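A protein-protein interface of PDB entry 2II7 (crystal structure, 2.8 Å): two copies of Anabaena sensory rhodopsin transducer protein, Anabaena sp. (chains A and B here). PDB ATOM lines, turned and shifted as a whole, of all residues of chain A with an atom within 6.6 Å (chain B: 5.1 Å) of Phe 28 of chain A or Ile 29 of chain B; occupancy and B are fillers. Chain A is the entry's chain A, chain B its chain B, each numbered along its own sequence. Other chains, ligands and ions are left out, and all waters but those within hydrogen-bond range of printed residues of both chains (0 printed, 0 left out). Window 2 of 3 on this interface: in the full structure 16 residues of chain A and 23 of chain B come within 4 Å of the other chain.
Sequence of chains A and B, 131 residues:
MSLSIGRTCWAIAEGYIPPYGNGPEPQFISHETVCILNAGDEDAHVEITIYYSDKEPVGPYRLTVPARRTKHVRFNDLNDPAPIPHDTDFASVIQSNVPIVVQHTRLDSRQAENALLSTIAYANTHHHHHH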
ATOM      1  N   PRO A  26     -11.582  21.443 -14.058  1.00  0.00           N
ATOM      2  CA  PRO A  26     -11.415  20.616 -15.256  1.00  0.00           C
ATOM      3  C   PRO A  26     -12.677  20.525 -16.096  1.00  0.00           C
ATOM      4  O   PRO A  26     -13.452  21.481 -16.176  1.00  0.00           O
ATOM      5  CB  PRO A  26     -11.004  19.265 -14.685  1.00  0.00           C
ATOM      6  CG  PRO A  26     -10.172  19.658 -13.519  1.00  0.00           C
ATOM      7  CD  PRO A  26     -10.993  20.776 -12.884  1.00  0.00           C
ATOM      8  N   GLN A  27     -12.877  19.360 -16.705  1.00  0.00           N
ATOM      9  CA  GLN A  27     -14.030  19.120 -17.567  1.00  0.00           C
ATOM     10  C   GLN A  27     -14.881  17.937 -17.083  1.00  0.00           C
ATOM     11  O   GLN A  27     -16.113  17.978 -17.135  1.00  0.00           O
ATOM     12  CB  GLN A  27     -13.535  18.853 -18.993  1.00  0.00           C
ATOM     13  CG  GLN A  27     -14.616  18.822 -20.062  1.00  0.00           C
ATOM     14  CD  GLN A  27     -15.233  20.187 -20.313  1.00  0.00           C
ATOM     15  OE1 GLN A  27     -15.904  20.744 -19.444  1.00  0.00           O
ATOM     16  NE2 GLN A  27     -15.000  20.737 -21.506  1.00  0.00           N
ATOM     17  N   PHE A  28     -14.209  16.891 -16.612  1.00  0.00           N
ATOM     18  CA  PHE A  28     -14.876  15.682 -16.136  1.00  0.00           C
ATOM     19  C   PHE A  28     -15.594  15.829 -14.800  1.00  0.00           C
ATOM     20  O   PHE A  28     -16.006  14.836 -14.194  1.00  0.00           O
ATOM     21  CB  PHE A  28     -13.868  14.533 -16.037  1.00  0.00           C
ATOM     22  CG  PHE A  28     -12.745  14.781 -15.062  1.00  0.00           C
ATOM     23  CD1 PHE A  28     -11.905  15.882 -15.202  1.00  0.00           C
ATOM     24  CD2 PHE A  28     -12.499  13.884 -14.027  1.00  0.00           C
ATOM     25  CE1 PHE A  28     -10.834  16.081 -14.323  1.00  0.00           C
ATOM     26  CE2 PHE A  28     -11.429  14.074 -13.142  1.00  0.00           C
ATOM     27  CZ  PHE A  28     -10.597  15.172 -13.292  1.00  0.00           C
ATOM     28  N   ILE A  29     -15.744  17.059 -14.330  1.00  0.00           N
ATOM     29  CA  ILE A  29     -16.431  17.265 -13.069  1.00  0.00           C
ATOM     30  C   ILE A  29     -17.822  17.804 -13.324  1.00  0.00           C
ATOM     31  O   ILE A  29     -18.023  18.669 -14.181  1.00  0.00           O
ATOM     32  CB  ILE A  29     -15.657  18.229 -12.139  1.00  0.00           C
ATOM     33  CG1 ILE A  29     -14.518  17.482 -11.445  1.00  0.00           C
ATOM     34  CG2 ILE A  29     -16.579  18.786 -11.076  1.00  0.00           C
ATOM     35  CD1 ILE A  29     -13.501  16.916 -12.390  1.00  0.00           C
ATOM     36  N   SER A  30     -18.780  17.266 -12.578  1.00  0.00           N
ATOM     37  CA  SER A  30     -20.175  17.665 -12.692  1.00  0.00           C
ATOM     38  C   SER A  30     -20.545  18.520 -11.491  1.00  0.00           C
ATOM     39  O   SER A  30     -19.828  18.538 -10.483  1.00  0.00           O
ATOM     40  CB  SER A  30     -21.070  16.424 -12.742  1.00  0.00           C
ATOM     41  OG  SER A  30     -20.806  15.575 -11.636  1.00  0.00           O
ATOM     42  N   ASN A 114     -16.956  12.742  -8.228  1.00  0.00           N
ATOM     43  CA  ASN A 114     -15.898  13.679  -8.589  1.00  0.00           C
ATOM     44  C   ASN A 114     -14.628  13.382  -7.812  1.00  0.00           C
ATOM     45  O   ASN A 114     -13.522  13.569  -8.318  1.00  0.00           O
ATOM     46  CB  ASN A 114     -16.343  15.122  -8.343  1.00  0.00           C
ATOM     47  CG  ASN A 114     -17.360  15.601  -9.373  1.00  0.00           C
ATOM     48  OD1 ASN A 114     -17.897  16.709  -9.270  1.00  0.00           O
ATOM     49  ND2 ASN A 114     -17.627  14.767 -10.377  1.00  0.00           N
ATOM     50  N   LEU A 116     -13.575  10.347  -6.713  1.00  0.00           N
ATOM     51  CA  LEU A 116     -12.981   9.167  -7.338  1.00  0.00           C
ATOM     52  C   LEU A 116     -12.368   9.497  -8.704  1.00  0.00           C
ATOM     53  O   LEU A 116     -11.311   8.968  -9.075  1.00  0.00           O
ATOM     54  CB  LEU A 116     -14.045   8.079  -7.493  1.00  0.00           C
ATOM     55  CG  LEU A 116     -14.692   7.590  -6.195  1.00  0.00           C
ATOM     56  CD1 LEU A 116     -15.837   6.624  -6.504  1.00  0.00           C
ATOM     57  CD2 LEU A 116     -13.632   6.916  -5.330  1.00  0.00           C
ATOM     58  N   LEU A 117     -13.038  10.379  -9.443  1.00  0.00           N
ATOM     59  CA  LEU A 117     -12.584  10.800 -10.765  1.00  0.00           C
ATOM     60  C   LEU A 117     -11.308  11.624 -10.628  1.00  0.00           C
ATOM     61  O   LEU A 117     -10.287  11.320 -11.260  1.00  0.00           O
ATOM     62  CB  LEU A 117     -13.679  11.631 -11.444  1.00  0.00           C
ATOM     63  CG  LEU A 117     -14.237  11.176 -12.800  1.00  0.00           C
ATOM     64  CD1 LEU A 117     -14.620   9.691 -12.788  1.00  0.00           C
ATOM     65  CD2 LEU A 117     -15.434  12.047 -13.131  1.00  0.00           C
ATOM     66  N   SER A 118     -11.374  12.668  -9.803  1.00  0.00           N
ATOM     67  CA  SER A 118     -10.222  13.527  -9.556  1.00  0.00           C
ATOM     68  C   SER A 118      -9.014  12.634  -9.352  1.00  0.00           C
ATOM     69  O   SER A 118      -8.102  12.628 -10.181  1.00  0.00           O
ATOM     70  CB  SER A 118     -10.462  14.371  -8.313  1.00  0.00           C
ATOM     71  OG  SER A 118     -11.618  15.158  -8.507  1.00  0.00           O
ATOM     72  N   THR A 119      -9.035  11.882  -8.251  1.00  0.00           N
ATOM     73  CA  THR A 119      -7.987  10.924  -7.900  1.00  0.00           C
ATOM     74  C   THR A 119      -7.275  10.400  -9.150  1.00  0.00           C
ATOM     75  O   THR A 119      -7.585   9.303  -9.635  1.00  0.00           O
ATOM     76  CB  THR A 119      -8.594   9.724  -7.146  1.00  0.00           C
ATOM     77  OG1 THR A 119      -9.268  10.192  -5.973  1.00  0.00           O
ATOM     78  CG2 THR A 119      -7.509   8.724  -6.745  1.00  0.00           C
ATOM     79  N   ILE A 120      -6.312  11.192  -9.639  1.00  0.00           N
ATOM     80  CA  ILE A 120      -5.529  10.908 -10.849  1.00  0.00           C
ATOM     81  C   ILE A 120      -6.270   9.952 -11.784  1.00  0.00           C
ATOM     82  O   ILE A 120      -6.868  10.474 -12.744  1.00  0.00           O
ATOM     83  CB  ILE A 120      -4.111  10.341 -10.506  1.00  0.00           C
ATOM     84  CG1 ILE A 120      -3.297  11.397  -9.765  1.00  0.00           C
ATOM     85  CG2 ILE A 120      -3.356   9.966 -11.779  1.00  0.00           C
ATOM     86  CD1 ILE A 120      -1.916  10.927  -9.410  1.00  0.00           C
ATOM     87  N   PRO B  18     -17.626  13.105 -21.555  1.00  0.00           N
ATOM     88  CA  PRO B  18     -16.573  14.133 -21.559  1.00  0.00           C
ATOM     89  C   PRO B  18     -15.594  14.069 -22.735  1.00  0.00           C
ATOM     90  O   PRO B  18     -15.198  12.992 -23.179  1.00  0.00           O
ATOM     91  CB  PRO B  18     -15.874  13.916 -20.215  1.00  0.00           C
ATOM     92  CG  PRO B  18     -16.963  13.380 -19.353  1.00  0.00           C
ATOM     93  CD  PRO B  18     -17.643  12.387 -20.268  1.00  0.00           C
ATOM     94  N   GLU B  25     -10.914   6.287 -24.343  1.00  0.00           N
ATOM     95  CA  GLU B  25     -11.448   7.041 -23.216  1.00  0.00           C
ATOM     96  C   GLU B  25     -10.786   6.593 -21.905  1.00  0.00           C
ATOM     97  O   GLU B  25     -10.719   5.398 -21.602  1.00  0.00           O
ATOM     98  CB  GLU B  25     -12.967   6.887 -23.128  1.00  0.00           C
ATOM     99  CG  GLU B  25     -13.470   5.485 -22.835  1.00  0.00           C
ATOM    100  CD  GLU B  25     -14.707   5.496 -21.944  1.00  0.00           C
ATOM    101  OE1 GLU B  25     -15.684   6.211 -22.261  1.00  0.00           O
ATOM    102  OE2 GLU B  25     -14.699   4.787 -20.918  1.00  0.00           O
ATOM    103  N   PRO B  26     -10.285   7.563 -21.116  1.00  0.00           N
ATOM    104  CA  PRO B  26      -9.599   7.402 -19.828  1.00  0.00           C
ATOM    105  C   PRO B  26     -10.460   6.882 -18.680  1.00  0.00           C
ATOM    106  O   PRO B  26     -11.686   7.029 -18.689  1.00  0.00           O
ATOM    107  CB  PRO B  26      -9.097   8.811 -19.521  1.00  0.00           C
ATOM    108  CG  PRO B  26      -9.161   9.524 -20.810  1.00  0.00           C
ATOM    109  CD  PRO B  26     -10.396   8.990 -21.442  1.00  0.00           C
ATOM    110  N   GLN B  27      -9.805   6.301 -17.675  1.00  0.00           N
ATOM    111  CA  GLN B  27     -10.513   5.784 -16.516  1.00  0.00           C
ATOM    112  C   GLN B  27     -11.057   6.921 -15.654  1.00  0.00           C
ATOM    113  O   GLN B  27     -11.972   6.714 -14.867  1.00  0.00           O
ATOM    114  CB  GLN B  27      -9.604   4.877 -15.686  1.00  0.00           C
ATOM    115  CG  GLN B  27      -9.388   3.477 -16.274  1.00  0.00           C
ATOM    116  CD  GLN B  27     -10.687   2.682 -16.416  1.00  0.00           C
ATOM    117  OE1 GLN B  27     -11.553   3.033 -17.218  1.00  0.00           O
ATOM    118  NE2 GLN B  27     -10.824   1.610 -15.633  1.00  0.00           N
ATOM    119  N   PHE B  28     -10.507   8.124 -15.802  1.00  0.00           N
ATOM    120  CA  PHE B  28     -10.991   9.263 -15.025  1.00  0.00           C
ATOM    121  C   PHE B  28     -12.095   9.994 -15.784  1.00  0.00           C
ATOM    122  O   PHE B  28     -12.214  11.223 -15.717  1.00  0.00           O
ATOM    123  CB  PHE B  28      -9.848  10.247 -14.695  1.00  0.00           C
ATOM    124  CG  PHE B  28      -9.051  10.709 -15.899  1.00  0.00           C
ATOM    125  CD1 PHE B  28      -7.899  10.025 -16.296  1.00  0.00           C
ATOM    126  CD2 PHE B  28      -9.473  11.803 -16.657  1.00  0.00           C
ATOM    127  CE1 PHE B  28      -7.186  10.417 -17.430  1.00  0.00           C
ATOM    128  CE2 PHE B  28      -8.767  12.203 -17.795  1.00  0.00           C
ATOM    129  CZ  PHE B  28      -7.621  11.507 -18.181  1.00  0.00           C
ATOM    130  N   ILE B  29     -12.921   9.235 -16.494  1.00  0.00           N
ATOM    131  CA  ILE B  29     -13.983   9.850 -17.265  1.00  0.00           C
ATOM    132  C   ILE B  29     -15.355   9.189 -17.094  1.00  0.00           C
ATOM    133  O   ILE B  29     -15.464   8.008 -16.769  1.00  0.00           O
ATOM    134  CB  ILE B  29     -13.584   9.889 -18.760  1.00  0.00           C
ATOM    135  CG1 ILE B  29     -13.969  11.240 -19.354  1.00  0.00           C
ATOM    136  CG2 ILE B  29     -14.242   8.752 -19.521  1.00  0.00           C
ATOM    137  CD1 ILE B  29     -13.285  12.403 -18.666  1.00  0.00           C
ATOM    138  N   SER B  30     -16.403   9.973 -17.323  1.00  0.00           N
ATOM    139  CA  SER B  30     -17.770   9.493 -17.192  1.00  0.00           C
ATOM    140  C   SER B  30     -18.096   8.294 -18.068  1.00  0.00           C
ATOM    141  O   SER B  30     -18.506   8.456 -19.221  1.00  0.00           O
ATOM    142  CB  SER B  30     -18.762  10.615 -17.517  1.00  0.00           C
ATOM    143  OG  SER B  30     -18.638  11.701 -16.619  1.00  0.00           O
ATOM    144  N   HIS B  31     -17.918   7.094 -17.524  1.00  0.00           N
ATOM    145  CA  HIS B  31     -18.259   5.868 -18.249  1.00  0.00           C
ATOM    146  C   HIS B  31     -19.776   5.700 -18.134  1.00  0.00           C
ATOM    147  O   HIS B  31     -20.271   4.623 -17.778  1.00  0.00           O
ATOM    148  CB  HIS B  31     -17.569   4.661 -17.611  1.00  0.00           C
ATOM    149  CG  HIS B  31     -16.097   4.606 -17.865  1.00  0.00           C
ATOM    150  ND1 HIS B  31     -15.320   5.739 -17.968  1.00  0.00           N
ATOM    151  CD2 HIS B  31     -15.259   3.555 -18.031  1.00  0.00           C
ATOM    152  CE1 HIS B  31     -14.066   5.389 -18.190  1.00  0.00           C
ATOM    153  NE2 HIS B  31     -14.002   4.070 -18.233  1.00  0.00           N
ATOM    154  N   ARG B 106     -23.283   7.030 -13.646  1.00  0.00           N
ATOM    155  CA  ARG B 106     -22.395   8.032 -14.231  1.00  0.00           C
ATOM    156  C   ARG B 106     -21.004   7.453 -14.383  1.00  0.00           C
ATOM    157  O   ARG B 106     -20.266   7.855 -15.278  1.00  0.00           O
ATOM    158  CB  ARG B 106     -22.351   9.313 -13.389  1.00  0.00           C
ATOM    159  CG  ARG B 106     -23.397  10.342 -13.807  1.00  0.00           C
ATOM    160  CD  ARG B 106     -23.704  11.319 -12.677  1.00  0.00           C
ATOM    161  NE  ARG B 106     -24.209  10.627 -11.490  1.00  0.00           N
ATOM    162  CZ  ARG B 106     -25.283   9.844 -11.487  1.00  0.00           C
ATOM    163  NH1 ARG B 106     -25.965   9.658 -12.608  1.00  0.00           N
ATOM    164  NH2 ARG B 106     -25.670   9.237 -10.371  1.00  0.00           N
ATOM    165  N   GLN B 111     -14.434   1.602 -11.912  1.00  0.00           N
ATOM    166  CA  GLN B 111     -13.760   2.890 -11.795  1.00  0.00           C
ATOM    167  C   GLN B 111     -13.721   3.120 -10.292  1.00  0.00           C
ATOM    168  O   GLN B 111     -12.748   3.643  -9.746  1.00  0.00           O
ATOM    169  CB  GLN B 111     -14.557   4.013 -12.450  1.00  0.00           C
ATOM    170  CG  GLN B 111     -14.644   3.953 -13.958  1.00  0.00           C
ATOM    171  CD  GLN B 111     -15.267   5.213 -14.530  1.00  0.00           C
ATOM    172  OE1 GLN B 111     -14.665   6.286 -14.501  1.00  0.00           O
ATOM    173  NE2 GLN B 111     -16.488   5.093 -15.037  1.00  0.00           N
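The backbone carbonyl oxygen (O) of Gln 27 of chain B sits close to the side-chain amide oxygen (OE1) of Gln 111 of chain B (2.8 Å).
The backbone carbonyl oxygen of Ile 29 of chain B lies within hydrogen-bond range of a ring nitrogen (ND1) of His 31 of chain B, 2.6 Å away.
The backbone carbonyl oxygen (O) of Ile 29 of chain B lies close to the side-chain amide oxygen (OE1) of Gln 111 of chain B.
The side-chain amide nitrogen (NE2) of Gln 111 of chain B sits close to a ring nitrogen (ND1) of His 31 of chain B (3.2 Å).
Among the printed residues, pairs that only touch across the chains: Phe 28 of chain A with Phe 28 of chain B, Phe 28 of chain A with Ile 29 of chain B, Leu 117 of chain A with Phe 28 of chain B, Ile 120 of chain A with Phe 28 of chain B and Leu 117 of chain A with Gln 111 of chain B.
Phe 28 of chain A touches just these residues of chain B: Phe 28 (3.2 Å) and Ile 29 (3.4 Å).
Of chain A, only Phe 28 (3.4 Å) comes within 4 Å of Ile 29 of chain B.
Of the printed residues of chain B, Ile 120 of chain A touches Phe 28 (3.6 Å).
Printed residues of chain B within 4 Å of Leu 117 of chain A: Phe 28 and Gln 111.
Printed residues of chain A within 4 Å of Gln 111 of chain B: Leu 117.
Of the printed residues of chain A, Phe 28 of chain B touches Phe 28 (3.2 Å), Leu 117 (3.6 Å) and Ile 120 (3.6 Å).
Thr 119 of chain A touches none of the printed residues of chain B.
The nearest residue of chain B that does not touch Phe 28 of chain A is Pro 18 of chain B (4.5 Å).
The nearest residue of chain A that does not touch Ile 29 of chain B is Leu 117 of chain A (4.1 Å).
The nearest printed residue of chain B that does not touch Leu 117 of chain A is Ile 29 of chain B (4.1 Å).
Hydrophobic or aromatic side chains of chain A that line the printed part of chain B: Phe 28 and Leu 117.
Of the 10 printed residues of chain B, 3 touch a printed residue of chain A.
Hydrophobic or aromatic side chains of chain B that line the printed part of chain A: Phe 28 and Ile 29.
Along chain B the printed residues that touch a printed residue of chain A span positions 28 to 111.
Among the printed residues, 5 pairs touch across the chains.
Phe 28 of chain B touches its own counterpart, Phe 28 of chain A.
Phe 28 of chain A touches Ile 29 of chain B, but with the chains exchanged Ile 29 of chain A does not touch Phe 28 of chain B (6.7 Å).
Of the 5 pairs that touch across the chains among the printed residues, 1 has its exchanged pair printed and touching as well.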
